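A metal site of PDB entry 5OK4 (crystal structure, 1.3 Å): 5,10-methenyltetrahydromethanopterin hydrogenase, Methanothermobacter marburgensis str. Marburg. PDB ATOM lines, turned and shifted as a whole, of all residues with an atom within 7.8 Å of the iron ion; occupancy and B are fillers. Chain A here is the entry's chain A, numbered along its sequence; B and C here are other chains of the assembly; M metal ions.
The backbone carbonyl oxygen (O) of Cys 255 sits at hydrogen-bond distance from the side-chain hydroxyl (OG1) of Thr 259, at 3.5 Å.
NE2 of His 187 of chain B is in hydrogen-bond range of OE1 of Glu 290 of chain C (2.8 Å).
N of Met 254 sits close to SG of Cys 252.
The side-chain sulfur of Cys 252 lies close to the backbone carbonyl oxygen of Gly 188 of chain B.
Of the 20 residues printed, 4 come within 4 Å of the iron ion.
Along chain A the residues within 4 Å of the iron ion span positions 249 to 255.
A ring nitrogen (ND1) of His 187 of chain B binds the iron ion (2.0 Å).
The backbone carbonyl oxygen (O) of Gly 249 binds the iron ion, 2.1 Å away.
SG of Cys 252 is bound to the iron ion, at 2.2 Å.
The iron ion is bound by SG of Cys 255 (2.3 Å).
The iron ion has four donor atoms within binding distance.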
ATOM      1  N   LEU A 247     -31.073  15.731   6.719  1.00  0.00           N
ATOM      2  CA  LEU A 247     -30.041  15.591   5.715  1.00  0.00           C
ATOM      3  C   LEU A 247     -29.389  16.914   5.339  1.00  0.00           C
ATOM      4  O   LEU A 247     -28.458  16.908   4.537  1.00  0.00           O
ATOM      5  CB  LEU A 247     -30.587  14.856   4.487  1.00  0.00           C
ATOM      6  CG  LEU A 247     -30.646  13.344   4.716  1.00  0.00           C
ATOM      7  CD1 LEU A 247     -31.705  12.751   3.846  1.00  0.00           C
ATOM      8  CD2 LEU A 247     -29.268  12.697   4.492  1.00  0.00           C
ATOM      9  N   LEU A 248     -29.818  18.045   5.913  1.00  0.00           N
ATOM     10  CA  LEU A 248     -29.208  19.320   5.544  1.00  0.00           C
ATOM     11  C   LEU A 248     -27.723  19.325   5.850  1.00  0.00           C
ATOM     12  O   LEU A 248     -26.893  19.604   4.985  1.00  0.00           O
ATOM     13  CB  LEU A 248     -29.867  20.499   6.258  1.00  0.00           C
ATOM     14  CG  LEU A 248     -31.022  21.181   5.566  1.00  0.00           C
ATOM     15  CD1 LEU A 248     -31.531  22.289   6.485  1.00  0.00           C
ATOM     16  CD2 LEU A 248     -30.682  21.763   4.189  1.00  0.00           C
ATOM     17  N   GLY A 249     -27.369  19.003   7.073  1.00  0.00           N
ATOM     18  CA  GLY A 249     -25.972  18.976   7.441  1.00  0.00           C
ATOM     19  C   GLY A 249     -25.161  18.082   6.528  1.00  0.00           C
ATOM     20  O   GLY A 249     -24.113  18.463   6.004  1.00  0.00           O
ATOM     21  N   PRO A 250     -25.635  16.861   6.330  1.00  0.00           N
ATOM     22  CA  PRO A 250     -24.914  15.926   5.468  1.00  0.00           C
ATOM     23  C   PRO A 250     -24.744  16.373   4.036  1.00  0.00           C
ATOM     24  O   PRO A 250     -23.893  15.806   3.338  1.00  0.00           O
ATOM     25  CB  PRO A 250     -25.773  14.657   5.540  1.00  0.00           C
ATOM     26  CG  PRO A 250     -26.302  14.706   6.947  1.00  0.00           C
ATOM     27  CD  PRO A 250     -26.618  16.159   7.177  1.00  0.00           C
ATOM     28  N   VAL A 251     -25.532  17.327   3.533  1.00  0.00           N
ATOM     29  CA  VAL A 251     -25.346  17.816   2.166  1.00  0.00           C
ATOM     30  C   VAL A 251     -24.663  19.176   2.094  1.00  0.00           C
ATOM     31  O   VAL A 251     -24.603  19.772   1.018  1.00  0.00           O
ATOM     32  CB  VAL A 251     -26.654  17.785   1.353  1.00  0.00           C
ATOM     33  CG1 VAL A 251     -27.310  16.405   1.410  1.00  0.00           C
ATOM     34  CG2 VAL A 251     -27.606  18.889   1.784  1.00  0.00           C
ATOM     35  N   CYS A 252     -24.125  19.681   3.207  1.00  0.00           N
ATOM     36  CA  CYS A 252     -23.424  20.957   3.155  1.00  0.00           C
ATOM     37  C   CYS A 252     -22.095  20.812   2.405  1.00  0.00           C
ATOM     38  O   CYS A 252     -21.659  19.718   2.057  1.00  0.00           O
ATOM     39  CB  CYS A 252     -23.185  21.529   4.555  1.00  0.00           C
ATOM     40  SG  CYS A 252     -21.756  20.894   5.408  1.00  0.00           S
ATOM     41  N   ASP A 253     -21.456  21.935   2.129  1.00  0.00           N
ATOM     42  CA  ASP A 253     -20.222  21.930   1.350  1.00  0.00           C
ATOM     43  C   ASP A 253     -19.101  21.168   2.046  1.00  0.00           C
ATOM     44  O   ASP A 253     -18.207  20.669   1.353  1.00  0.00           O
ATOM     45  CB  ASP A 253     -19.813  23.364   1.011  1.00  0.00           C
ATOM     46  CG  ASP A 253     -20.779  23.996   0.029  1.00  0.00           C
ATOM     47  OD1 ASP A 253     -21.798  24.540   0.463  1.00  0.00           O
ATOM     48  OD2 ASP A 253     -20.530  23.920  -1.173  1.00  0.00           O
ATOM     49  N   MET A 254     -19.141  21.048   3.375  1.00  0.00           N
ATOM     50  CA  MET A 254     -18.118  20.298   4.098  1.00  0.00           C
ATOM     51  C   MET A 254     -18.334  18.804   4.056  1.00  0.00           C
ATOM     52  O   MET A 254     -17.382  18.036   4.147  1.00  0.00           O
ATOM     53  CB  MET A 254     -18.063  20.723   5.553  1.00  0.00           C
ATOM     54  CG  MET A 254     -17.944  22.200   5.810  1.00  0.00           C
ATOM     55  SD  MET A 254     -16.447  22.868   5.191  1.00  0.00           S
ATOM     56  CE  MET A 254     -15.232  21.931   6.063  1.00  0.00           C
ATOM     57  N   CYS A 255     -19.583  18.378   3.982  1.00  0.00           N
ATOM     58  CA  CYS A 255     -19.929  16.976   4.180  1.00  0.00           C
ATOM     59  C   CYS A 255     -20.357  16.258   2.927  1.00  0.00           C
ATOM     60  O   CYS A 255     -20.280  15.020   2.876  1.00  0.00           O
ATOM     61  CB  CYS A 255     -21.127  16.870   5.126  1.00  0.00           C
ATOM     62  SG  CYS A 255     -20.810  17.513   6.761  1.00  0.00           S
ATOM     63  N   SER A 256     -20.847  16.986   1.938  1.00  0.00           N
ATOM     64  CA  SER A 256     -21.598  16.377   0.867  1.00  0.00           C
ATOM     65  C   SER A 256     -20.783  15.343   0.129  1.00  0.00           C
ATOM     66  O   SER A 256     -21.322  14.344  -0.322  1.00  0.00           O
ATOM     67  CB  SER A 256     -22.088  17.463  -0.083  1.00  0.00           C
ATOM     68  OG  SER A 256     -22.836  16.850  -1.114  1.00  0.00           O
ATOM     69  N   THR A 259     -21.277  12.037   1.808  1.00  0.00           N
ATOM     70  CA  THR A 259     -22.653  11.587   1.648  1.00  0.00           C
ATOM     71  C   THR A 259     -22.898  11.130   0.221  1.00  0.00           C
ATOM     72  O   THR A 259     -23.583  10.134   0.000  1.00  0.00           O
ATOM     73  CB  THR A 259     -23.586  12.737   2.023  1.00  0.00           C
ATOM     74  OG1 THR A 259     -23.190  13.202   3.300  1.00  0.00           O
ATOM     75  CG2 THR A 259     -25.052  12.293   2.040  1.00  0.00           C
ATOM     76  N   LYS B 186     -19.775  22.764  13.228  1.00  0.00           N
ATOM     77  CA  LYS B 186     -19.965  21.561  12.431  1.00  0.00           C
ATOM     78  C   LYS B 186     -19.984  21.902  10.948  1.00  0.00           C
ATOM     79  O   LYS B 186     -18.954  21.907  10.272  1.00  0.00           O
ATOM     80  CB  LYS B 186     -21.246  20.839  12.870  1.00  0.00           C
ATOM     81  CG  LYS B 186     -21.189  20.320  14.301  1.00  0.00           C
ATOM     82  CD  LYS B 186     -21.974  19.016  14.465  1.00  0.00           C
ATOM     83  CE  LYS B 186     -23.170  19.197  15.372  1.00  0.00           C
ATOM     84  NZ  LYS B 186     -23.306  18.046  16.311  1.00  0.00           N
ATOM     85  N   HIS B 187     -21.152  22.262  10.452  1.00  0.00           N
ATOM     86  CA  HIS B 187     -21.401  22.349   9.025  1.00  0.00           C
ATOM     87  C   HIS B 187     -21.037  23.725   8.501  1.00  0.00           C
ATOM     88  O   HIS B 187     -20.952  24.698   9.239  1.00  0.00           O
ATOM     89  CB  HIS B 187     -22.875  22.064   8.789  1.00  0.00           C
ATOM     90  CG  HIS B 187     -23.257  20.730   9.309  1.00  0.00           C
ATOM     91  ND1 HIS B 187     -22.915  19.562   8.655  1.00  0.00           N
ATOM     92  CD2 HIS B 187     -23.843  20.366  10.462  1.00  0.00           C
ATOM     93  CE1 HIS B 187     -23.309  18.538   9.391  1.00  0.00           C
ATOM     94  NE2 HIS B 187     -23.867  19.004  10.494  1.00  0.00           N
ATOM     95  N   GLY B 188     -20.816  23.801   7.206  1.00  0.00           N
ATOM     96  CA  GLY B 188     -20.441  25.072   6.619  1.00  0.00           C
ATOM     97  C   GLY B 188     -20.568  25.059   5.124  1.00  0.00           C
ATOM     98  O   GLY B 188     -20.640  24.013   4.488  1.00  0.00           O
ATOM     99  N   ASP B 189     -20.516  26.254   4.568  1.00  0.00           N
ATOM    100  CA  ASP B 189     -20.757  26.459   3.163  1.00  0.00           C
ATOM    101  C   ASP B 189     -19.499  26.764   2.387  1.00  0.00           C
ATOM    102  O   ASP B 189     -19.538  26.767   1.160  1.00  0.00           O
ATOM    103  CB  ASP B 189     -21.737  27.611   2.976  1.00  0.00           C
ATOM    104  CG  ASP B 189     -23.023  27.379   3.742  1.00  0.00           C
ATOM    105  OD1 ASP B 189     -23.456  26.195   3.828  1.00  0.00           O
ATOM    106  OD2 ASP B 189     -23.591  28.358   4.298  1.00  0.00           O
ATOM    107  N   TYR C 269     -12.277  10.717   2.025  1.00  0.00           N
ATOM    108  CA  TYR C 269     -12.760  11.948   2.634  1.00  0.00           C
ATOM    109  C   TYR C 269     -11.872  12.358   3.795  1.00  0.00           C
ATOM    110  O   TYR C 269     -11.449  13.513   3.888  1.00  0.00           O
ATOM    111  CB  TYR C 269     -14.196  11.705   3.105  1.00  0.00           C
ATOM    112  CG  TYR C 269     -14.826  12.874   3.806  1.00  0.00           C
ATOM    113  CD1 TYR C 269     -15.238  14.010   3.100  1.00  0.00           C
ATOM    114  CD2 TYR C 269     -15.020  12.848   5.175  1.00  0.00           C
ATOM    115  CE1 TYR C 269     -15.828  15.052   3.744  1.00  0.00           C
ATOM    116  CE2 TYR C 269     -15.618  13.898   5.841  1.00  0.00           C
ATOM    117  CZ  TYR C 269     -16.023  14.985   5.119  1.00  0.00           C
ATOM    118  OH  TYR C 269     -16.613  16.017   5.762  1.00  0.00           O
ATOM    119  N   MET C 286     -16.357  13.653  12.903  1.00  0.00           N
ATOM    120  CA  MET C 286     -17.649  14.174  13.319  1.00  0.00           C
ATOM    121  C   MET C 286     -18.569  14.364  12.125  1.00  0.00           C
ATOM    122  O   MET C 286     -19.755  14.040  12.190  1.00  0.00           O
ATOM    123  CB  MET C 286     -17.456  15.471  14.086  1.00  0.00           C
ATOM    124  CG  MET C 286     -18.759  16.171  14.342  1.00  0.00           C
ATOM    125  SD  MET C 286     -19.032  17.400  13.073  1.00  0.00           S
ATOM    126  CE  MET C 286     -18.084  18.689  13.896  1.00  0.00           C
ATOM    127  N   MET C 287     -18.025  14.866  11.010  1.00  0.00           N
ATOM    128  CA  MET C 287     -18.857  15.021   9.816  1.00  0.00           C
ATOM    129  C   MET C 287     -19.270  13.662   9.267  1.00  0.00           C
ATOM    130  O   MET C 287     -20.427  13.453   8.909  1.00  0.00           O
ATOM    131  CB  MET C 287     -18.106  15.799   8.749  1.00  0.00           C
ATOM    132  CG  MET C 287     -17.820  17.276   9.107  1.00  0.00           C
ATOM    133  SD  MET C 287     -17.096  18.255   7.772  1.00  0.00           S
ATOM    134  CE  MET C 287     -15.422  17.585   7.800  1.00  0.00           C
ATOM    135  N   GLU C 290     -22.179  11.912  11.221  1.00  0.00           N
ATOM    136  CA  GLU C 290     -23.515  12.417  10.963  1.00  0.00           C
ATOM    137  C   GLU C 290     -23.975  12.028   9.576  1.00  0.00           C
ATOM    138  O   GLU C 290     -25.131  11.641   9.370  1.00  0.00           O
ATOM    139  CB  GLU C 290     -23.576  13.937  11.195  1.00  0.00           C
ATOM    140  CG  GLU C 290     -24.967  14.511  10.979  1.00  0.00           C
ATOM    141  CD  GLU C 290     -25.061  15.992  11.209  1.00  0.00           C
ATOM    142  OE1 GLU C 290     -24.129  16.557  11.841  1.00  0.00           O
ATOM    143  OE2 GLU C 290     -26.053  16.599  10.760  1.00  0.00           O
ATOM    144  N   SER C 291     -23.071  12.113   8.595  1.00  0.00           N
ATOM    145  CA  SER C 291     -23.408  11.756   7.215  1.00  0.00           C
ATOM    146  C   SER C 291     -23.807  10.298   7.117  1.00  0.00           C
ATOM    147  O   SER C 291     -24.863   9.954   6.557  1.00  0.00           O
ATOM    148  CB  SER C 291     -22.188  12.023   6.346  1.00  0.00           C
ATOM    149  OG  SER C 291     -22.347  11.518   5.039  1.00  0.00           O
HETATM  150 FE    FE M   1     -22.289  19.234   6.788  1.00  0.00          FE
